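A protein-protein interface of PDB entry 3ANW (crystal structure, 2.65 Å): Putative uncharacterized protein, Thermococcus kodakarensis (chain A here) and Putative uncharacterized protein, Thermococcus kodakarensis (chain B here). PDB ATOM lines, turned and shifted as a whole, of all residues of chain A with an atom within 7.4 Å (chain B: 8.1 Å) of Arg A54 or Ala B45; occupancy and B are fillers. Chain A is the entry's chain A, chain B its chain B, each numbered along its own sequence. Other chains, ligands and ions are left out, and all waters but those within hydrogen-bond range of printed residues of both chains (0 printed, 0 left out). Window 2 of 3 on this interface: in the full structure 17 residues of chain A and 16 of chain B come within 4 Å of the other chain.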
ATOM      1  N   ALA A  41      17.889 -18.546   4.630  1.00  0.00           N
ATOM      2  CA  ALA A  41      16.531 -18.277   4.147  1.00  0.00           C
ATOM      3  C   ALA A  41      15.428 -18.421   5.211  1.00  0.00           C
ATOM      4  O   ALA A  41      14.428 -17.690   5.187  1.00  0.00           O
ATOM      5  CB  ALA A  41      16.214 -19.164   2.947  1.00  0.00           C
ATOM      6  N   SER A  44      15.255 -15.723   7.934  1.00  0.00           N
ATOM      7  CA  SER A  44      14.780 -14.426   7.423  1.00  0.00           C
ATOM      8  C   SER A  44      13.257 -14.428   7.237  1.00  0.00           C
ATOM      9  O   SER A  44      12.606 -13.397   7.398  1.00  0.00           O
ATOM     10  CB  SER A  44      15.450 -14.076   6.090  1.00  0.00           C
ATOM     11  OG  SER A  44      16.851 -13.892   6.241  1.00  0.00           O
ATOM     12  N   ARG A  45      12.701 -15.584   6.871  1.00  0.00           N
ATOM     13  CA  ARG A  45      11.261 -15.741   6.660  1.00  0.00           C
ATOM     14  C   ARG A  45      10.567 -15.474   7.992  1.00  0.00           C
ATOM     15  O   ARG A  45       9.681 -14.617   8.088  1.00  0.00           O
ATOM     16  CB  ARG A  45      10.951 -17.168   6.207  1.00  0.00           C
ATOM     17  CG  ARG A  45       9.468 -17.457   6.080  1.00  0.00           C
ATOM     18  CD  ARG A  45       9.162 -18.932   6.338  1.00  0.00           C
ATOM     19  NE  ARG A  45       9.453 -19.336   7.721  1.00  0.00           N
ATOM     20  CZ  ARG A  45       8.553 -19.375   8.713  1.00  0.00           C
ATOM     21  NH1 ARG A  45       7.284 -19.027   8.494  1.00  0.00           N
ATOM     22  NH2 ARG A  45       8.918 -19.783   9.926  1.00  0.00           N
ATOM     23  N   GLU A  49      11.489 -10.742   6.881  1.00  0.00           N
ATOM     24  CA  GLU A  49      12.018  -9.938   5.765  1.00  0.00           C
ATOM     25  C   GLU A  49      11.624 -10.609   4.477  1.00  0.00           C
ATOM     26  O   GLU A  49      12.293 -11.535   4.035  1.00  0.00           O
ATOM     27  CB  GLU A  49      13.538  -9.786   5.788  1.00  0.00           C
ATOM     28  CG  GLU A  49      14.083  -8.959   6.929  1.00  0.00           C
ATOM     29  CD  GLU A  49      14.832  -9.817   7.909  1.00  0.00           C
ATOM     30  OE1 GLU A  49      15.987  -9.462   8.249  1.00  0.00           O
ATOM     31  OE2 GLU A  49      14.271 -10.867   8.311  1.00  0.00           O
ATOM     32  N   ASP A  50      10.515 -10.170   3.893  1.00  0.00           N
ATOM     33  CA  ASP A  50      10.053 -10.757   2.639  1.00  0.00           C
ATOM     34  C   ASP A  50      11.104 -10.509   1.561  1.00  0.00           C
ATOM     35  O   ASP A  50      11.268 -11.318   0.657  1.00  0.00           O
ATOM     36  CB  ASP A  50       8.707 -10.157   2.206  1.00  0.00           C
ATOM     37  CG  ASP A  50       7.600 -10.393   3.224  1.00  0.00           C
ATOM     38  OD1 ASP A  50       6.906 -11.437   3.142  1.00  0.00           O
ATOM     39  OD2 ASP A  50       7.418  -9.518   4.101  1.00  0.00           O
ATOM     40  N   VAL A  51      11.836  -9.404   1.688  1.00  0.00           N
ATOM     41  CA  VAL A  51      12.866  -9.040   0.716  1.00  0.00           C
ATOM     42  C   VAL A  51      14.156  -9.829   0.896  1.00  0.00           C
ATOM     43  O   VAL A  51      14.613 -10.482  -0.038  1.00  0.00           O
ATOM     44  CB  VAL A  51      13.168  -7.531   0.733  1.00  0.00           C
ATOM     45  CG1 VAL A  51      14.027  -7.165  -0.476  1.00  0.00           C
ATOM     46  CG2 VAL A  51      11.865  -6.733   0.725  1.00  0.00           C
ATOM     47  N   GLU A  52      14.733  -9.776   2.089  1.00  0.00           N
ATOM     48  CA  GLU A  52      15.961 -10.510   2.367  1.00  0.00           C
ATOM     49  C   GLU A  52      15.786 -12.002   2.096  1.00  0.00           C
ATOM     50  O   GLU A  52      16.721 -12.684   1.678  1.00  0.00           O
ATOM     51  CB  GLU A  52      16.415 -10.280   3.814  1.00  0.00           C
ATOM     52  CG  GLU A  52      17.411 -11.319   4.332  1.00  0.00           C
ATOM     53  CD  GLU A  52      18.363 -10.784   5.403  1.00  0.00           C
ATOM     54  OE1 GLU A  52      18.168  -9.629   5.860  1.00  0.00           O
ATOM     55  OE2 GLU A  52      19.321 -11.517   5.775  1.00  0.00           O
ATOM     56  N   GLU A  53      14.571 -12.489   2.301  1.00  0.00           N
ATOM     57  CA  GLU A  53      14.241 -13.893   2.083  1.00  0.00           C
ATOM     58  C   GLU A  53      14.142 -14.201   0.588  1.00  0.00           C
ATOM     59  O   GLU A  53      14.755 -15.148   0.100  1.00  0.00           O
ATOM     60  CB  GLU A  53      12.906 -14.212   2.768  1.00  0.00           C
ATOM     61  CG  GLU A  53      12.365 -15.590   2.490  1.00  0.00           C
ATOM     62  CD  GLU A  53      10.851 -15.626   2.403  1.00  0.00           C
ATOM     63  OE1 GLU A  53      10.219 -14.598   2.014  1.00  0.00           O
ATOM     64  OE2 GLU A  53      10.299 -16.713   2.705  1.00  0.00           O
ATOM     65  N   ARG A  54      13.359 -13.390  -0.117  1.00  0.00           N
ATOM     66  CA  ARG A  54      13.134 -13.531  -1.547  1.00  0.00           C
ATOM     67  C   ARG A  54      14.468 -13.642  -2.280  1.00  0.00           C
ATOM     68  O   ARG A  54      14.588 -14.376  -3.262  1.00  0.00           O
ATOM     69  CB  ARG A  54      12.353 -12.321  -2.066  1.00  0.00           C
ATOM     70  CG  ARG A  54      11.456 -12.598  -3.264  1.00  0.00           C
ATOM     71  CD  ARG A  54      10.894 -11.301  -3.868  1.00  0.00           C
ATOM     72  NE  ARG A  54      10.501 -10.342  -2.835  1.00  0.00           N
ATOM     73  CZ  ARG A  54       9.392 -10.423  -2.099  1.00  0.00           C
ATOM     74  NH1 ARG A  54       8.535 -11.423  -2.285  1.00  0.00           N
ATOM     75  NH2 ARG A  54       9.167  -9.535  -1.127  1.00  0.00           N
ATOM     76  N   LEU A  55      15.469 -12.919  -1.783  1.00  0.00           N
ATOM     77  CA  LEU A  55      16.799 -12.931  -2.380  1.00  0.00           C
ATOM     78  C   LEU A  55      17.560 -14.209  -2.059  1.00  0.00           C
ATOM     79  O   LEU A  55      18.211 -14.771  -2.929  1.00  0.00           O
ATOM     80  CB  LEU A  55      17.602 -11.700  -1.953  1.00  0.00           C
ATOM     81  CG  LEU A  55      17.126 -10.363  -2.521  1.00  0.00           C
ATOM     82  CD1 LEU A  55      17.918  -9.246  -1.911  1.00  0.00           C
ATOM     83  CD2 LEU A  55      17.272 -10.336  -4.021  1.00  0.00           C
ATOM     84  N   TYR A  56      17.476 -14.674  -0.817  1.00  0.00           N
ATOM     85  CA  TYR A  56      18.151 -15.913  -0.430  1.00  0.00           C
ATOM     86  C   TYR A  56      17.586 -17.106  -1.180  1.00  0.00           C
ATOM     87  O   TYR A  56      18.299 -18.071  -1.465  1.00  0.00           O
ATOM     88  CB  TYR A  56      18.029 -16.165   1.065  1.00  0.00           C
ATOM     89  CG  TYR A  56      19.077 -15.465   1.877  1.00  0.00           C
ATOM     90  CD1 TYR A  56      18.733 -14.445   2.762  1.00  0.00           C
ATOM     91  CD2 TYR A  56      20.422 -15.822   1.763  1.00  0.00           C
ATOM     92  CE1 TYR A  56      19.705 -13.797   3.517  1.00  0.00           C
ATOM     93  CE2 TYR A  56      21.404 -15.182   2.512  1.00  0.00           C
ATOM     94  CZ  TYR A  56      21.038 -14.172   3.388  1.00  0.00           C
ATOM     95  OH  TYR A  56      21.993 -13.554   4.154  1.00  0.00           O
ATOM     96  N   LEU A  57      16.293 -17.043  -1.470  1.00  0.00           N
ATOM     97  CA  LEU A  57      15.627 -18.106  -2.203  1.00  0.00           C
ATOM     98  C   LEU A  57      15.971 -18.051  -3.684  1.00  0.00           C
ATOM     99  O   LEU A  57      16.257 -19.073  -4.287  1.00  0.00           O
ATOM    100  CB  LEU A  57      14.112 -18.026  -2.013  1.00  0.00           C
ATOM    101  CG  LEU A  57      13.581 -18.282  -0.604  1.00  0.00           C
ATOM    102  CD1 LEU A  57      12.057 -18.363  -0.640  1.00  0.00           C
ATOM    103  CD2 LEU A  57      14.175 -19.575  -0.066  1.00  0.00           C
ATOM    104  N   ALA A  58      15.945 -16.857  -4.264  1.00  0.00           N
ATOM    105  CA  ALA A  58      16.250 -16.695  -5.681  1.00  0.00           C
ATOM    106  C   ALA A  58      17.677 -17.115  -6.013  1.00  0.00           C
ATOM    107  O   ALA A  58      17.948 -17.532  -7.131  1.00  0.00           O
ATOM    108  CB  ALA A  58      16.011 -15.254  -6.120  1.00  0.00           C
ATOM    109  N   GLN A  59      18.587 -16.967  -5.053  1.00  0.00           N
ATOM    110  CA  GLN A  59      19.982 -17.348  -5.241  1.00  0.00           C
ATOM    111  C   GLN A  59      20.091 -18.852  -5.244  1.00  0.00           C
ATOM    112  O   GLN A  59      20.895 -19.416  -5.963  1.00  0.00           O
ATOM    113  CB  GLN A  59      20.858 -16.805  -4.111  1.00  0.00           C
ATOM    114  CG  GLN A  59      21.216 -15.342  -4.203  1.00  0.00           C
ATOM    115  CD  GLN A  59      22.214 -14.927  -3.144  1.00  0.00           C
ATOM    116  OE1 GLN A  59      21.837 -14.599  -2.026  1.00  0.00           O
ATOM    117  NE2 GLN A  59      23.493 -14.946  -3.487  1.00  0.00           N
ATOM    118  N   LEU A  60      19.295 -19.482  -4.387  1.00  0.00           N
ATOM    119  CA  LEU A  60      19.254 -20.928  -4.231  1.00  0.00           C
ATOM    120  C   LEU A  60      18.700 -21.587  -5.486  1.00  0.00           C
ATOM    121  O   LEU A  60      19.179 -22.641  -5.878  1.00  0.00           O
ATOM    122  CB  LEU A  60      18.406 -21.299  -3.009  1.00  0.00           C
ATOM    123  CG  LEU A  60      18.127 -22.774  -2.726  1.00  0.00           C
ATOM    124  CD1 LEU A  60      19.342 -23.453  -2.146  1.00  0.00           C
ATOM    125  CD2 LEU A  60      16.986 -22.873  -1.760  1.00  0.00           C
ATOM    126  N   MET B  20      14.141   2.985  -4.669  1.00  0.00           N
ATOM    127  CA  MET B  20      12.923   3.616  -4.152  1.00  0.00           C
ATOM    128  C   MET B  20      12.962   3.730  -2.620  1.00  0.00           C
ATOM    129  O   MET B  20      12.471   4.706  -2.052  1.00  0.00           O
ATOM    130  CB  MET B  20      11.668   2.825  -4.542  1.00  0.00           C
ATOM    131  CG  MET B  20      11.457   2.583  -6.029  1.00  0.00           C
ATOM    132  SD  MET B  20      11.676   4.013  -7.093  1.00  0.00           S
ATOM    133  CE  MET B  20      10.625   5.254  -6.284  1.00  0.00           C
ATOM    134  N   LYS B  21      13.544   2.736  -1.955  1.00  0.00           N
ATOM    135  CA  LYS B  21      13.622   2.747  -0.498  1.00  0.00           C
ATOM    136  C   LYS B  21      15.024   2.384   0.036  1.00  0.00           C
ATOM    137  O   LYS B  21      15.826   1.789  -0.676  1.00  0.00           O
ATOM    138  CB  LYS B  21      12.515   1.852   0.087  1.00  0.00           C
ATOM    139  CG  LYS B  21      12.324   0.529  -0.633  1.00  0.00           C
ATOM    140  CD  LYS B  21      10.972  -0.123  -0.333  1.00  0.00           C
ATOM    141  CE  LYS B  21       9.810   0.633  -0.983  1.00  0.00           C
ATOM    142  NZ  LYS B  21       8.665  -0.281  -1.337  1.00  0.00           N
ATOM    143  N   PHE B  23      17.033   0.383   1.247  1.00  0.00           N
ATOM    144  CA  PHE B  23      17.677  -0.931   1.233  1.00  0.00           C
ATOM    145  C   PHE B  23      19.205  -0.876   1.280  1.00  0.00           C
ATOM    146  O   PHE B  23      19.835  -0.228   0.443  1.00  0.00           O
ATOM    147  CB  PHE B  23      17.236  -1.720   0.002  1.00  0.00           C
ATOM    148  CG  PHE B  23      17.476  -3.183   0.123  1.00  0.00           C
ATOM    149  CD1 PHE B  23      16.618  -3.973   0.890  1.00  0.00           C
ATOM    150  CD2 PHE B  23      18.585  -3.771  -0.482  1.00  0.00           C
ATOM    151  CE1 PHE B  23      16.862  -5.335   1.057  1.00  0.00           C
ATOM    152  CE2 PHE B  23      18.844  -5.127  -0.325  1.00  0.00           C
ATOM    153  CZ  PHE B  23      17.984  -5.918   0.447  1.00  0.00           C
ATOM    154  N   TRP B  37      19.129 -10.911 -12.157  1.00  0.00           N
ATOM    155  CA  TRP B  37      18.284 -11.678 -11.263  1.00  0.00           C
ATOM    156  C   TRP B  37      17.921 -10.883 -10.012  1.00  0.00           C
ATOM    157  O   TRP B  37      16.829 -11.037  -9.466  1.00  0.00           O
ATOM    158  CB  TRP B  37      18.987 -12.978 -10.874  1.00  0.00           C
ATOM    159  CG  TRP B  37      20.127 -12.805  -9.925  1.00  0.00           C
ATOM    160  CD1 TRP B  37      21.437 -12.710 -10.241  1.00  0.00           C
ATOM    161  CD2 TRP B  37      20.052 -12.721  -8.495  1.00  0.00           C
ATOM    162  NE1 TRP B  37      22.194 -12.572  -9.103  1.00  0.00           N
ATOM    163  CE2 TRP B  37      21.364 -12.574  -8.017  1.00  0.00           C
ATOM    164  CE3 TRP B  37      19.001 -12.756  -7.575  1.00  0.00           C
ATOM    165  CZ2 TRP B  37      21.658 -12.459  -6.662  1.00  0.00           C
ATOM    166  CZ3 TRP B  37      19.290 -12.644  -6.226  1.00  0.00           C
ATOM    167  CH2 TRP B  37      20.611 -12.497  -5.781  1.00  0.00           C
ATOM    168  N   ALA B  39      17.826  -7.730 -10.025  1.00  0.00           N
ATOM    169  CA  ALA B  39      17.046  -6.624 -10.543  1.00  0.00           C
ATOM    170  C   ALA B  39      15.585  -7.016 -10.578  1.00  0.00           C
ATOM    171  O   ALA B  39      14.732  -6.228 -10.194  1.00  0.00           O
ATOM    172  CB  ALA B  39      17.514  -6.252 -11.935  1.00  0.00           C
ATOM    173  N   ARG B  40      15.288  -8.233 -11.032  1.00  0.00           N
ATOM    174  CA  ARG B  40      13.895  -8.660 -11.085  1.00  0.00           C
ATOM    175  C   ARG B  40      13.312  -8.911  -9.690  1.00  0.00           C
ATOM    176  O   ARG B  40      12.153  -8.588  -9.442  1.00  0.00           O
ATOM    177  CB  ARG B  40      13.693  -9.873 -12.018  1.00  0.00           C
ATOM    178  CG  ARG B  40      13.882 -11.242 -11.400  1.00  0.00           C
ATOM    179  CD  ARG B  40      12.638 -12.102 -11.581  1.00  0.00           C
ATOM    180  NE  ARG B  40      12.368 -12.393 -12.988  1.00  0.00           N
ATOM    181  CZ  ARG B  40      11.876 -13.546 -13.445  1.00  0.00           C
ATOM    182  NH1 ARG B  40      11.588 -14.536 -12.609  1.00  0.00           N
ATOM    183  NH2 ARG B  40      11.698 -13.724 -14.750  1.00  0.00           N
ATOM    184  N   GLU B  41      14.132  -9.417  -8.771  1.00  0.00           N
ATOM    185  CA  GLU B  41      13.663  -9.687  -7.411  1.00  0.00           C
ATOM    186  C   GLU B  41      13.349  -8.414  -6.628  1.00  0.00           C
ATOM    187  O   GLU B  41      12.284  -8.320  -6.022  1.00  0.00           O
ATOM    188  CB  GLU B  41      14.642 -10.568  -6.617  1.00  0.00           C
ATOM    189  CG  GLU B  41      14.717 -12.033  -7.074  1.00  0.00           C
ATOM    190  CD  GLU B  41      13.388 -12.784  -7.007  1.00  0.00           C
ATOM    191  OE1 GLU B  41      12.682 -12.862  -8.035  1.00  0.00           O
ATOM    192  OE2 GLU B  41      13.064 -13.327  -5.935  1.00  0.00           O
ATOM    193  N   LEU B  42      14.271  -7.450  -6.621  1.00  0.00           N
ATOM    194  CA  LEU B  42      14.042  -6.189  -5.910  1.00  0.00           C
ATOM    195  C   LEU B  42      12.950  -5.362  -6.594  1.00  0.00           C
ATOM    196  O   LEU B  42      12.258  -4.588  -5.931  1.00  0.00           O
ATOM    197  CB  LEU B  42      15.328  -5.370  -5.796  1.00  0.00           C
ATOM    198  CG  LEU B  42      16.442  -5.914  -4.897  1.00  0.00           C
ATOM    199  CD1 LEU B  42      17.780  -5.318  -5.300  1.00  0.00           C
ATOM    200  CD2 LEU B  42      16.132  -5.635  -3.441  1.00  0.00           C
ATOM    201  N   TRP B  43      12.784  -5.526  -7.909  1.00  0.00           N
ATOM    202  CA  TRP B  43      11.747  -4.786  -8.627  1.00  0.00           C
ATOM    203  C   TRP B  43      10.381  -5.291  -8.175  1.00  0.00           C
ATOM    204  O   TRP B  43       9.499  -4.498  -7.869  1.00  0.00           O
ATOM    205  CB  TRP B  43      11.883  -4.971 -10.144  1.00  0.00           C
ATOM    206  CG  TRP B  43      10.878  -4.178 -10.956  1.00  0.00           C
ATOM    207  CD1 TRP B  43      10.403  -2.928 -10.674  1.00  0.00           C
ATOM    208  CD2 TRP B  43      10.302  -4.547 -12.219  1.00  0.00           C
ATOM    209  NE1 TRP B  43       9.591  -2.489 -11.689  1.00  0.00           N
ATOM    210  CE2 TRP B  43       9.508  -3.459 -12.649  1.00  0.00           C
ATOM    211  CE3 TRP B  43      10.390  -5.686 -13.034  1.00  0.00           C
ATOM    212  CZ2 TRP B  43       8.799  -3.472 -13.864  1.00  0.00           C
ATOM    213  CZ3 TRP B  43       9.686  -5.701 -14.247  1.00  0.00           C
ATOM    214  CH2 TRP B  43       8.901  -4.597 -14.648  1.00  0.00           C
ATOM    215  N   GLU B  44      10.216  -6.614  -8.155  1.00  0.00           N
ATOM    216  CA  GLU B  44       8.971  -7.263  -7.737  1.00  0.00           C
ATOM    217  C   GLU B  44       8.491  -6.818  -6.358  1.00  0.00           C
ATOM    218  O   GLU B  44       7.289  -6.856  -6.075  1.00  0.00           O
ATOM    219  CB  GLU B  44       9.140  -8.782  -7.718  1.00  0.00           C
ATOM    220  CG  GLU B  44       8.873  -9.485  -9.045  1.00  0.00           C
ATOM    221  CD  GLU B  44       9.091 -10.996  -8.956  1.00  0.00           C
ATOM    222  OE1 GLU B  44       9.200 -11.640 -10.032  1.00  0.00           O
ATOM    223  OE2 GLU B  44       9.165 -11.535  -7.817  1.00  0.00           O
ATOM    224  N   ALA B  45       9.428  -6.417  -5.503  1.00  0.00           N
ATOM    225  CA  ALA B  45       9.104  -5.973  -4.149  1.00  0.00           C
ATOM    226  C   ALA B  45       9.309  -4.461  -3.967  1.00  0.00           C
ATOM    227  O   ALA B  45       9.775  -4.005  -2.926  1.00  0.00           O
ATOM    228  CB  ALA B  45       9.932  -6.771  -3.124  1.00  0.00           C
ATOM    229  N   GLY B  46       8.997  -3.696  -5.006  1.00  0.00           N
ATOM    230  CA  GLY B  46       9.124  -2.246  -4.957  1.00  0.00           C
ATOM    231  C   GLY B  46      10.317  -1.579  -4.270  1.00  0.00           C
ATOM    232  O   GLY B  46      10.188  -0.431  -3.804  1.00  0.00           O
ATOM    233  N   VAL B  47      11.458  -2.274  -4.179  1.00  0.00           N
ATOM    234  CA  VAL B  47      12.661  -1.694  -3.562  1.00  0.00           C
ATOM    235  C   VAL B  47      13.374  -0.822  -4.599  1.00  0.00           C
ATOM    236  O   VAL B  47      13.994   0.182  -4.260  1.00  0.00           O
ATOM    237  CB  VAL B  47      13.645  -2.777  -3.040  1.00  0.00           C
ATOM    238  CG1 VAL B  47      14.936  -2.141  -2.546  1.00  0.00           C
ATOM    239  CG2 VAL B  47      13.016  -3.564  -1.930  1.00  0.00           C
ATOM    240  N   VAL B  48      13.268  -1.213  -5.864  1.00  0.00           N
ATOM    241  CA  VAL B  48      13.902  -0.466  -6.944  1.00  0.00           C
ATOM    242  C   VAL B  48      12.936  -0.333  -8.099  1.00  0.00           C
ATOM    243  O   VAL B  48      11.849  -0.905  -8.082  1.00  0.00           O
ATOM    244  CB  VAL B  48      15.210  -1.150  -7.466  1.00  0.00           C
ATOM    245  CG1 VAL B  48      16.232  -1.269  -6.363  1.00  0.00           C
ATOM    246  CG2 VAL B  48      14.913  -2.509  -8.048  1.00  0.00           C
ATOM    247  N   ASN B  99       2.731  -2.410 -10.815  1.00  0.00           N
ATOM    248  CA  ASN B  99       2.118  -2.292  -9.473  1.00  0.00           C
ATOM    249  C   ASN B  99       1.787  -0.867  -8.946  1.00  0.00           C
ATOM    250  O   ASN B  99       2.676   0.007  -8.875  1.00  0.00           O
ATOM    251  CB  ASN B  99       2.995  -3.041  -8.430  1.00  0.00           C
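The backbone carbonyl oxygen (O) of Arg A54 sits close to the side-chain carboxylate (OE2) of Glu B41, 3.3 Å away.
O of Asp A50 lies close to NH2 of Arg A54, at 3.3 Å.
O of Leu B42 lies within hydrogen-bond range of N of Val B47, at 3.0 Å.
Phe B23 touches Val A51 (CE1 to CG1, 3.7 Å).
Val A51 touches Leu B42 (CG1 to CD2, 3.9 Å).
Ala B45 touches Arg A54 (CB to NH2, 3.5 Å).
Leu A55 touches Trp B37.
Leu A55 touches Glu B41 (CD2 to CB, 3.7 Å).
Glu B41 touches Ala A58.
Gln A59 touches Trp B37.
Arg A54 touches just these residues of chain B: Glu B41 (3.2 Å) and Ala B45 (3.5 Å).
Ala B45 touches just one residue of chain A: Arg A54 (3.5 Å).
Of the printed residues of chain B, Gln A59 touches Trp B37.
Of the printed residues of chain A, Glu B41 touches Arg A54, Leu A55 and Ala A58.
Printed residues of chain A within 4 Å of Trp B37: Leu A55 (3.8 Å) and Gln A59 (3.3 Å).
Printed residues of chain A within 4 Å of Leu B42: Val A51.
Ala B39 touches none of the printed residues of chain A.
Of the 15 printed residues of chain A, 5 touch a printed residue of chain B.
Hydrophobic or aromatic side chains of chain A within 4 Å of the printed part of chain B: Val A51, Leu A55 and Ala A58.
Along chain A the printed residues that touch a printed residue of chain B span positions 51 to 59.
Hydrophobic or aromatic side chains of chain B within 4 Å of the printed part of chain A: Phe B23, Trp B37, Leu B42 and Ala B45.
Along chain B the printed residues that touch a printed residue of chain A span positions 23 to 45.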
